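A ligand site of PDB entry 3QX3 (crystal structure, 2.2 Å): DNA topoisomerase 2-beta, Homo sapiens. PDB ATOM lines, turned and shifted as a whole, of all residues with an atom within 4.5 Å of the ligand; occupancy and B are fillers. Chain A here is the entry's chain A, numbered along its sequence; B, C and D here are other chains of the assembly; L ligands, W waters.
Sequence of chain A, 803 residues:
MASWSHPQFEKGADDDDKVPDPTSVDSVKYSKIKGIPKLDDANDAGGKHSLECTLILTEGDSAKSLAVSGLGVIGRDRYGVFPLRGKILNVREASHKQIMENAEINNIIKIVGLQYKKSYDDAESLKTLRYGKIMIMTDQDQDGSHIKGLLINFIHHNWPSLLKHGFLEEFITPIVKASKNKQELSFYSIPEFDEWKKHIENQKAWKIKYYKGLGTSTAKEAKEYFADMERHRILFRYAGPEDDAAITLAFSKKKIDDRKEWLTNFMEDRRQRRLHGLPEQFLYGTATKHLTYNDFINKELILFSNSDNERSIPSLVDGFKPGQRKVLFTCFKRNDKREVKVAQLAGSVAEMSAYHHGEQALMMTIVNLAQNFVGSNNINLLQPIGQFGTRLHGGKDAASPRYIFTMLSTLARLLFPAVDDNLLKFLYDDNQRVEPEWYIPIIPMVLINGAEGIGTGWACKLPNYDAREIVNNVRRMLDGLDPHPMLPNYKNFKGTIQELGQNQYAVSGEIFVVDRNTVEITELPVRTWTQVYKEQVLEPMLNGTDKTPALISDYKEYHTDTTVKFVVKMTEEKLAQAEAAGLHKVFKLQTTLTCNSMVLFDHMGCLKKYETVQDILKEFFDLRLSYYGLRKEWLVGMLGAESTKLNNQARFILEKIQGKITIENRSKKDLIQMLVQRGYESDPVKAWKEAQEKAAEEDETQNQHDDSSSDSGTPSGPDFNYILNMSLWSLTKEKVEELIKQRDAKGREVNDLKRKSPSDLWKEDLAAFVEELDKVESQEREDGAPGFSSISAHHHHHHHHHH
Water W6 lies within hydrogen-bond range of an oxygen (O6) of the ligand (2.6 Å), OP1 of DG 2 of chain D (2.6 Å), O3' of DT 1 of chain D (2.8 Å) and the backbone NH (N) of Asp 61 (2.9 Å). Water W7 lies within hydrogen-bond range of N7 of DG 5 of chain B and an oxygen (O13) of the ligand. Water W5 bridges O12 of the ligand (2.7 Å) and SD of Met 364 (3.5 Å). Water W2 lies within hydrogen-bond range of an oxygen (O3) of the ligand (3.3 Å) and OP2 of DT 1 of chain D (3.4 Å). Water W3 bridges N4 of DC 6 of chain B (3.0 Å) and O13 of the ligand (3.4 Å). Water W1 lies within hydrogen-bond range of N6 of DA 4 of chain B (3.2 Å) and O11 of the ligand (3.4 Å).
The backbone NH (N) of Asp 61 lies within hydrogen-bond range of an oxygen (O6) of the ligand (3.1 Å). The side-chain carboxylate of Asp 61 lies within hydrogen-bond range of an oxygen (O6) of the ligand, 2.5 Å away. An oxygen (O13) of the ligand is in hydrogen-bond range of O6 of DG 5 of chain B, at 2.7 Å. The guanidinium group (NE) of Arg 85 lies close to an oxygen (O2) of the ligand, 3.2 Å away.
O4' of DG 5 of chain B sits at hydrogen-bond distance from the guanidinium group of Arg 85 (3.3 Å). The backbone NH of Gly 60 is in hydrogen-bond range of the backbone carbonyl oxygen of Leu 84, 2.7 Å away. O3' of DC 8 of chain C lies close to OE2 of Glu 59 (2.6 Å).
SD of Met 364 lies close to O11 of the ligand. An oxygen (O1) of the ligand lies close to N3 of DA 4 of chain B (3.4 Å). An oxygen (O8) of the ligand sits close to N4 of DC 8 of chain C. O5 of the ligand lies close to O4' of DG 2 of chain D, 3.4 Å away. Gly 60 touches the ligand (CA to O7, 3.0 Å). OE1 of Gln 360 touches O10 of the ligand, 3.5 Å away. DT 1 of chain D touches the ligand (O2 to C20, 3.3 Å). Hydrophobic or aromatic side chains that line the ligand: Met 364. Within 4 Å of the ligand: Gly 60, Asp 61, Arg 85, Gln 360, Met 364, DA 4 of chain B, DG 5 of chain B, DC 8 of chain C, DT 1 of chain D and DG 2 of chain D.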
ATOM      1  N   GLU A  59     -11.105 -18.833 -20.167  1.00  0.00           N
ATOM      2  CA  GLU A  59     -10.166 -19.547 -19.302  1.00  0.00           C
ATOM      3  C   GLU A  59     -10.870 -20.750 -18.671  1.00  0.00           C
ATOM      4  O   GLU A  59     -11.464 -20.641 -17.589  1.00  0.00           O
ATOM      5  CB  GLU A  59      -9.604 -18.611 -18.224  1.00  0.00           C
ATOM      6  CG  GLU A  59      -8.466 -19.231 -17.424  1.00  0.00           C
ATOM      7  CD  GLU A  59      -7.847 -18.290 -16.387  1.00  0.00           C
ATOM      8  OE1 GLU A  59      -8.187 -17.089 -16.376  1.00  0.00           O
ATOM      9  OE2 GLU A  59      -7.003 -18.762 -15.597  1.00  0.00           O
ATOM     10  N   GLY A  60     -10.834 -21.896 -19.352  1.00  0.00           N
ATOM     11  CA  GLY A  60     -11.408 -23.126 -18.827  1.00  0.00           C
ATOM     12  C   GLY A  60     -12.891 -23.292 -19.100  1.00  0.00           C
ATOM     13  O   GLY A  60     -13.587 -22.338 -19.487  1.00  0.00           O
ATOM     14  N   ASP A  61     -13.394 -24.504 -18.872  1.00  0.00           N
ATOM     15  CA  ASP A  61     -14.756 -24.916 -19.255  1.00  0.00           C
ATOM     16  C   ASP A  61     -15.823 -24.234 -18.416  1.00  0.00           C
ATOM     17  O   ASP A  61     -16.886 -23.884 -18.909  1.00  0.00           O
ATOM     18  CB  ASP A  61     -14.896 -26.446 -19.204  1.00  0.00           C
ATOM     19  CG  ASP A  61     -13.838 -27.162 -20.047  1.00  0.00           C
ATOM     20  OD1 ASP A  61     -12.685 -27.320 -19.581  1.00  0.00           O
ATOM     21  OD2 ASP A  61     -14.154 -27.547 -21.192  1.00  0.00           O
ATOM     22  N   LEU A  84     -10.277 -22.457 -23.380  1.00  0.00           N
ATOM     23  CA  LEU A  84      -8.865 -22.820 -23.291  1.00  0.00           C
ATOM     24  C   LEU A  84      -8.615 -23.627 -22.008  1.00  0.00           C
ATOM     25  O   LEU A  84      -9.248 -23.385 -20.988  1.00  0.00           O
ATOM     26  CB  LEU A  84      -8.023 -21.553 -23.293  1.00  0.00           C
ATOM     27  CG  LEU A  84      -8.269 -20.630 -24.475  1.00  0.00           C
ATOM     28  CD1 LEU A  84      -7.656 -19.261 -24.239  1.00  0.00           C
ATOM     29  CD2 LEU A  84      -7.709 -21.263 -25.735  1.00  0.00           C
ATOM     30  N   ARG A  85      -7.691 -24.583 -22.068  1.00  0.00           N
ATOM     31  CA  ARG A  85      -7.370 -25.433 -20.918  1.00  0.00           C
ATOM     32  C   ARG A  85      -6.205 -24.864 -20.098  1.00  0.00           C
ATOM     33  O   ARG A  85      -5.359 -25.603 -19.624  1.00  0.00           O
ATOM     34  CB  ARG A  85      -6.985 -26.843 -21.368  1.00  0.00           C
ATOM     35  CG  ARG A  85      -7.957 -27.499 -22.344  1.00  0.00           C
ATOM     36  CD  ARG A  85      -7.542 -28.923 -22.671  1.00  0.00           C
ATOM     37  NE  ARG A  85      -6.231 -29.003 -23.316  1.00  0.00           N
ATOM     38  CZ  ARG A  85      -5.736 -30.113 -23.871  1.00  0.00           C
ATOM     39  NH1 ARG A  85      -6.454 -31.226 -23.858  1.00  0.00           N
ATOM     40  NH2 ARG A  85      -4.540 -30.109 -24.436  1.00  0.00           N
ATOM     41  N   GLY A  86      -6.155 -23.546 -19.947  1.00  0.00           N
ATOM     42  CA  GLY A  86      -5.076 -22.898 -19.198  1.00  0.00           C
ATOM     43  C   GLY A  86      -4.020 -22.265 -20.099  1.00  0.00           C
ATOM     44  O   GLY A  86      -4.339 -21.674 -21.127  1.00  0.00           O
ATOM     45  N   GLN A 360      -5.238 -28.206  -6.137  1.00  0.00           N
ATOM     46  CA  GLN A 360      -4.426 -29.289  -6.684  1.00  0.00           C
ATOM     47  C   GLN A 360      -2.926 -28.925  -6.710  1.00  0.00           C
ATOM     48  O   GLN A 360      -2.081 -29.792  -6.487  1.00  0.00           O
ATOM     49  CB  GLN A 360      -4.916 -29.733  -8.059  1.00  0.00           C
ATOM     50  CG  GLN A 360      -6.313 -30.366  -8.052  1.00  0.00           C
ATOM     51  CD  GLN A 360      -6.391 -31.640  -7.220  1.00  0.00           C
ATOM     52  OE1 GLN A 360      -5.512 -32.507  -7.300  1.00  0.00           O
ATOM     53  NE2 GLN A 360      -7.456 -31.759  -6.412  1.00  0.00           N
ATOM     54  N   MET A 364       0.175 -30.920  -4.558  1.00  0.00           N
ATOM     55  CA  MET A 364       1.483 -31.315  -5.083  1.00  0.00           C
ATOM     56  C   MET A 364       2.640 -30.746  -4.244  1.00  0.00           C
ATOM     57  O   MET A 364       3.656 -31.405  -4.034  1.00  0.00           O
ATOM     58  CB  MET A 364       1.639 -30.943  -6.556  1.00  0.00           C
ATOM     59  CG  MET A 364       0.703 -31.716  -7.494  1.00  0.00           C
ATOM     60  SD  MET A 364       0.948 -31.278  -9.245  1.00  0.00           S
ATOM     61  CE  MET A 364       2.472 -32.153  -9.630  1.00  0.00           C
ATOM     62  P    DA B   4      -0.967 -40.104 -18.953  1.00  0.00           P
ATOM     63  OP1  DA B   4      -0.175 -41.014 -19.826  1.00  0.00           O
ATOM     64  OP2  DA B   4      -0.510 -39.771 -17.593  1.00  0.00           O
ATOM     65  O5'  DA B   4      -1.174 -38.699 -19.714  1.00  0.00           O
ATOM     66  C5'  DA B   4      -1.731 -38.644 -21.022  1.00  0.00           C
ATOM     67  C4'  DA B   4      -2.237 -37.226 -21.259  1.00  0.00           C
ATOM     68  O4'  DA B   4      -3.392 -37.007 -20.415  1.00  0.00           O
ATOM     69  C3'  DA B   4      -1.235 -36.107 -20.950  1.00  0.00           C
ATOM     70  O3'  DA B   4      -0.498 -35.804 -22.155  1.00  0.00           O
ATOM     71  C2'  DA B   4      -2.145 -34.964 -20.502  1.00  0.00           C
ATOM     72  C1'  DA B   4      -3.388 -35.666 -19.945  1.00  0.00           C
ATOM     73  N9   DA B   4      -3.438 -35.655 -18.481  1.00  0.00           N
ATOM     74  C8   DA B   4      -2.462 -36.075 -17.610  1.00  0.00           C
ATOM     75  N7   DA B   4      -2.775 -35.933 -16.350  1.00  0.00           N
ATOM     76  C5   DA B   4      -4.043 -35.369 -16.376  1.00  0.00           C
ATOM     77  C6   DA B   4      -4.928 -34.960 -15.369  1.00  0.00           C
ATOM     78  N6   DA B   4      -4.662 -35.081 -14.048  1.00  0.00           N
ATOM     79  N1   DA B   4      -6.112 -34.441 -15.751  1.00  0.00           N
ATOM     80  C2   DA B   4      -6.387 -34.335 -17.054  1.00  0.00           C
ATOM     81  N3   DA B   4      -5.622 -34.677 -18.093  1.00  0.00           N
ATOM     82  C4   DA B   4      -4.464 -35.195 -17.689  1.00  0.00           C
ATOM     83  P    DG B   5       0.825 -34.883 -22.118  1.00  0.00           P
ATOM     84  OP1  DG B   5       1.706 -35.317 -23.226  1.00  0.00           O
ATOM     85  OP2  DG B   5       1.362 -34.862 -20.733  1.00  0.00           O
ATOM     86  O5'  DG B   5       0.269 -33.417 -22.444  1.00  0.00           O
ATOM     87  C5'  DG B   5      -0.441 -33.198 -23.655  1.00  0.00           C
ATOM     88  C4'  DG B   5      -0.761 -31.731 -23.832  1.00  0.00           C
ATOM     89  O4'  DG B   5      -1.856 -31.404 -22.928  1.00  0.00           O
ATOM     90  C3'  DG B   5       0.355 -30.726 -23.505  1.00  0.00           C
ATOM     91  O3'  DG B   5       1.180 -30.439 -24.649  1.00  0.00           O
ATOM     92  C2'  DG B   5      -0.487 -29.507 -23.180  1.00  0.00           C
ATOM     93  C1'  DG B   5      -1.603 -30.140 -22.371  1.00  0.00           C
ATOM     94  N9   DG B   5      -1.324 -30.251 -20.935  1.00  0.00           N
ATOM     95  C8   DG B   5      -0.847 -31.319 -20.197  1.00  0.00           C
ATOM     96  N7   DG B   5      -0.720 -31.053 -18.928  1.00  0.00           N
ATOM     97  C5   DG B   5      -1.164 -29.735 -18.799  1.00  0.00           C
ATOM     98  C6   DG B   5      -1.283 -28.894 -17.672  1.00  0.00           C
ATOM     99  O6   DG B   5      -1.018 -29.131 -16.494  1.00  0.00           O
ATOM    100  N1   DG B   5      -1.762 -27.624 -18.018  1.00  0.00           N
ATOM    101  C2   DG B   5      -2.085 -27.217 -19.299  1.00  0.00           C
ATOM    102  N2   DG B   5      -2.538 -25.974 -19.480  1.00  0.00           N
ATOM    103  N3   DG B   5      -1.975 -28.010 -20.342  1.00  0.00           N
ATOM    104  C4   DG B   5      -1.524 -29.234 -20.031  1.00  0.00           C
ATOM    105  P    DC B   6       2.672 -29.896 -24.450  1.00  0.00           P
ATOM    106  OP1  DC B   6       3.283 -29.751 -25.787  1.00  0.00           O
ATOM    107  OP2  DC B   6       3.339 -30.731 -23.431  1.00  0.00           O
ATOM    108  O5'  DC B   6       2.483 -28.449 -23.771  1.00  0.00           O
ATOM    109  C5'  DC B   6       1.765 -27.395 -24.386  1.00  0.00           C
ATOM    110  C4'  DC B   6       1.578 -26.233 -23.432  1.00  0.00           C
ATOM    111  O4'  DC B   6       0.724 -26.651 -22.333  1.00  0.00           O
ATOM    112  C3'  DC B   6       2.825 -25.629 -22.772  1.00  0.00           C
ATOM    113  O3'  DC B   6       3.320 -24.591 -23.594  1.00  0.00           O
ATOM    114  C2'  DC B   6       2.231 -24.957 -21.549  1.00  0.00           C
ATOM    115  C1'  DC B   6       1.074 -25.886 -21.195  1.00  0.00           C
ATOM    116  N1   DC B   6       1.411 -26.828 -20.082  1.00  0.00           N
ATOM    117  C2   DC B   6       1.291 -26.304 -18.802  1.00  0.00           C
ATOM    118  O2   DC B   6       0.934 -25.132 -18.722  1.00  0.00           O
ATOM    119  N3   DC B   6       1.559 -27.091 -17.731  1.00  0.00           N
ATOM    120  C4   DC B   6       1.939 -28.352 -17.932  1.00  0.00           C
ATOM    121  N4   DC B   6       2.196 -29.090 -16.844  1.00  0.00           N
ATOM    122  C5   DC B   6       2.080 -28.899 -19.246  1.00  0.00           C
ATOM    123  C6   DC B   6       1.805 -28.112 -20.299  1.00  0.00           C
ATOM    124  P    DC C   8      -3.682 -21.132 -10.296  1.00  0.00           P
ATOM    125  OP1  DC C   8      -4.430 -19.930  -9.853  1.00  0.00           O
ATOM    126  OP2  DC C   8      -4.014 -22.445  -9.686  1.00  0.00           O
ATOM    127  O5'  DC C   8      -3.806 -21.305 -11.871  1.00  0.00           O
ATOM    128  C5'  DC C   8      -3.856 -20.149 -12.715  1.00  0.00           C
ATOM    129  C4'  DC C   8      -4.109 -20.608 -14.139  1.00  0.00           C
ATOM    130  O4'  DC C   8      -2.950 -21.336 -14.565  1.00  0.00           O
ATOM    131  C3'  DC C   8      -5.241 -21.609 -14.309  1.00  0.00           C
ATOM    132  O3'  DC C   8      -6.489 -20.974 -14.403  1.00  0.00           O
ATOM    133  C2'  DC C   8      -4.855 -22.222 -15.646  1.00  0.00           C
ATOM    134  C1'  DC C   8      -3.343 -22.325 -15.491  1.00  0.00           C
ATOM    135  N1   DC C   8      -2.906 -23.679 -15.065  1.00  0.00           N
ATOM    136  C2   DC C   8      -2.575 -24.545 -16.098  1.00  0.00           C
ATOM    137  O2   DC C   8      -2.659 -24.108 -17.263  1.00  0.00           O
ATOM    138  N3   DC C   8      -2.158 -25.802 -15.802  1.00  0.00           N
ATOM    139  C4   DC C   8      -2.092 -26.205 -14.536  1.00  0.00           C
ATOM    140  N4   DC C   8      -1.700 -27.472 -14.328  1.00  0.00           N
ATOM    141  C5   DC C   8      -2.430 -25.326 -13.452  1.00  0.00           C
ATOM    142  C6   DC C   8      -2.826 -24.084 -13.761  1.00  0.00           C
ATOM    143  P    DT D   1      -9.735 -26.776 -10.163  1.00  0.00           P
ATOM    144  OP1  DT D   1      -9.353 -27.816  -9.205  1.00  0.00           O
ATOM    145  OP2  DT D   1      -9.357 -25.354  -9.999  1.00  0.00           O
ATOM    146  O5'  DT D   1      -9.302 -27.311 -11.611  1.00  0.00           O
ATOM    147  C5'  DT D   1      -9.445 -26.564 -12.813  1.00  0.00           C
ATOM    148  C4'  DT D   1      -9.897 -27.522 -13.897  1.00  0.00           C
ATOM    149  O4'  DT D   1      -8.971 -28.620 -13.988  1.00  0.00           O
ATOM    150  C3'  DT D   1     -11.249 -28.168 -13.575  1.00  0.00           C
ATOM    151  O3'  DT D   1     -12.215 -27.530 -14.408  1.00  0.00           O
ATOM    152  C2'  DT D   1     -11.071 -29.668 -13.854  1.00  0.00           C
ATOM    153  C1'  DT D   1      -9.643 -29.781 -14.403  1.00  0.00           C
ATOM    154  N1   DT D   1      -8.846 -30.903 -13.819  1.00  0.00           N
ATOM    155  C2   DT D   1      -8.206 -31.803 -14.627  1.00  0.00           C
ATOM    156  O2   DT D   1      -8.242 -31.766 -15.835  1.00  0.00           O
ATOM    157  N3   DT D   1      -7.480 -32.759 -13.976  1.00  0.00           N
ATOM    158  C4   DT D   1      -7.339 -32.914 -12.623  1.00  0.00           C
ATOM    159  O4   DT D   1      -6.666 -33.812 -12.138  1.00  0.00           O
ATOM    160  C5   DT D   1      -8.040 -31.931 -11.820  1.00  0.00           C
ATOM    161  C7   DT D   1      -7.970 -31.986 -10.323  1.00  0.00           C
ATOM    162  C6   DT D   1      -8.744 -30.977 -12.450  1.00  0.00           C
ATOM    163  P    DG D   2     -13.777 -27.928 -14.300  1.00  0.00           P
ATOM    164  OP1  DG D   2     -14.561 -26.761 -14.747  1.00  0.00           O
ATOM    165  OP2  DG D   2     -14.005 -28.525 -12.967  1.00  0.00           O
ATOM    166  O5'  DG D   2     -13.918 -29.129 -15.344  1.00  0.00           O
ATOM    167  C5'  DG D   2     -13.493 -28.978 -16.698  1.00  0.00           C
ATOM    168  C4'  DG D   2     -13.721 -30.273 -17.474  1.00  0.00           C
ATOM    169  O4'  DG D   2     -12.745 -31.280 -17.117  1.00  0.00           O
ATOM    170  C3'  DG D   2     -15.085 -30.928 -17.267  1.00  0.00           C
ATOM    171  O3'  DG D   2     -15.464 -31.483 -18.494  1.00  0.00           O
ATOM    172  C2'  DG D   2     -14.793 -32.007 -16.217  1.00  0.00           C
ATOM    173  C1'  DG D   2     -13.387 -32.434 -16.600  1.00  0.00           C
ATOM    174  N9   DG D   2     -12.575 -32.906 -15.475  1.00  0.00           N
ATOM    175  C8   DG D   2     -12.644 -32.528 -14.161  1.00  0.00           C
ATOM    176  N7   DG D   2     -11.766 -33.129 -13.400  1.00  0.00           N
ATOM    177  C5   DG D   2     -11.072 -33.960 -14.283  1.00  0.00           C
ATOM    178  C6   DG D   2     -10.008 -34.864 -14.051  1.00  0.00           C
ATOM    179  O6   DG D   2      -9.445 -35.112 -12.970  1.00  0.00           O
ATOM    180  N1   DG D   2      -9.610 -35.503 -15.229  1.00  0.00           N
ATOM    181  C2   DG D   2     -10.158 -35.294 -16.457  1.00  0.00           C
ATOM    182  N2   DG D   2      -9.633 -36.018 -17.480  1.00  0.00           N
ATOM    183  N3   DG D   2     -11.167 -34.466 -16.686  1.00  0.00           N
ATOM    184  C4   DG D   2     -11.566 -33.832 -15.562  1.00  0.00           C
HETATM  185  C1  LIG L   1      -4.538 -32.107 -21.325  1.00  0.00           C
HETATM  186  O1  LIG L   1      -3.971 -32.564 -20.133  1.00  0.00           O
HETATM  187  C2  LIG L   1      -4.607 -30.455 -19.916  1.00  0.00           C
HETATM  188  O2  LIG L   1      -4.539 -30.719 -21.241  1.00  0.00           O
HETATM  189  C3  LIG L   1      -4.988 -29.188 -19.168  1.00  0.00           C
HETATM  190  O3  LIG L   1      -5.715 -27.538 -13.151  1.00  0.00           O
HETATM  191  C4  LIG L   1      -5.002 -29.208 -17.687  1.00  0.00           C
HETATM  192  O4  LIG L   1      -5.621 -25.706 -14.688  1.00  0.00           O
HETATM  193  C5  LIG L   1      -5.414 -27.891 -16.877  1.00  0.00           C
HETATM  194  O5  LIG L   1     -10.275 -29.141 -18.095  1.00  0.00           O
HETATM  195  C6  LIG L   1      -5.118 -27.968 -15.423  1.00  0.00           C
HETATM  196  O6  LIG L   1     -11.137 -26.401 -17.826  1.00  0.00           O
HETATM  197  C7  LIG L   1      -5.534 -26.882 -14.439  1.00  0.00           C
HETATM  198  O7  LIG L   1      -9.252 -24.348 -17.095  1.00  0.00           O
HETATM  199  C8  LIG L   1      -5.594 -28.987 -13.346  1.00  0.00           C
HETATM  200  O8  LIG L   1      -3.328 -30.273 -14.834  1.00  0.00           O
HETATM  201  C9  LIG L   1      -5.487 -29.250 -14.829  1.00  0.00           C
HETATM  202  O9  LIG L   1      -3.558 -31.470 -13.064  1.00  0.00           O
HETATM  203  C10 LIG L   1      -4.649 -30.377 -15.407  1.00  0.00           C
HETATM  204  O10 LIG L   1      -3.438 -33.297 -10.033  1.00  0.00           O
HETATM  205  C11 LIG L   1      -4.647 -30.403 -16.959  1.00  0.00           C
HETATM  206  O11 LIG L   1      -1.256 -33.456 -11.014  1.00  0.00           O
HETATM  207  C12 LIG L   1      -4.267 -31.628 -17.696  1.00  0.00           C
HETATM  208  O12 LIG L   1       0.367 -32.152 -13.196  1.00  0.00           O
HETATM  209  C13 LIG L   1      -4.263 -31.605 -19.225  1.00  0.00           C
HETATM  210  O13 LIG L   1      -0.989 -31.611 -15.393  1.00  0.00           O
HETATM  211  C14 LIG L   1      -6.902 -27.497 -17.121  1.00  0.00           C
HETATM  212  C15 LIG L   1      -7.904 -28.550 -17.507  1.00  0.00           C
HETATM  213  C16 LIG L   1      -9.357 -28.179 -17.746  1.00  0.00           C
HETATM  214  C17 LIG L   1      -9.800 -26.741 -17.617  1.00  0.00           C
HETATM  215  C18 LIG L   1      -8.804 -25.680 -17.233  1.00  0.00           C
HETATM  216  C19 LIG L   1      -7.366 -26.057 -16.979  1.00  0.00           C
HETATM  217  C20 LIG L   1      -9.813 -30.419 -18.413  1.00  0.00           C
HETATM  218  C21 LIG L   1      -8.457 -23.364 -16.516  1.00  0.00           C
HETATM  219  C22 LIG L   1      -2.811 -31.576 -14.177  1.00  0.00           C
HETATM  220  C23 LIG L   1      -3.092 -32.465 -12.167  1.00  0.00           C
HETATM  221  C24 LIG L   1      -3.826 -32.355 -10.994  1.00  0.00           C
HETATM  222  C25 LIG L   1      -2.003 -33.403  -9.824  1.00  0.00           C
HETATM  223  C26 LIG L   1      -1.578 -32.431 -11.847  1.00  0.00           C
HETATM  224  C27 LIG L   1      -0.999 -32.352 -13.264  1.00  0.00           C
HETATM  225  C28 LIG L   1      -1.612 -31.321 -14.106  1.00  0.00           C
HETATM  226  C29 LIG L   1      -1.664 -34.572  -8.951  1.00  0.00           C
HETATM  227  O   HOH W   1      -2.261 -36.393 -12.480  1.00  0.00           O
HETATM  228  O   HOH W   2      -6.478 -24.686 -11.580  1.00  0.00           O
HETATM  229  O   HOH W   3       2.106 -32.068 -16.637  1.00  0.00           O
HETATM  230  O   HOH W   4     -11.460 -23.849 -14.552  1.00  0.00           O
HETATM  231  O   HOH W   5       1.635 -29.902 -12.399  1.00  0.00           O
HETATM  232  O   HOH W   6     -12.799 -25.398 -16.125  1.00  0.00           O
HETATM  233  O   HOH W   7      -0.275 -33.162 -17.436  1.00  0.00           O
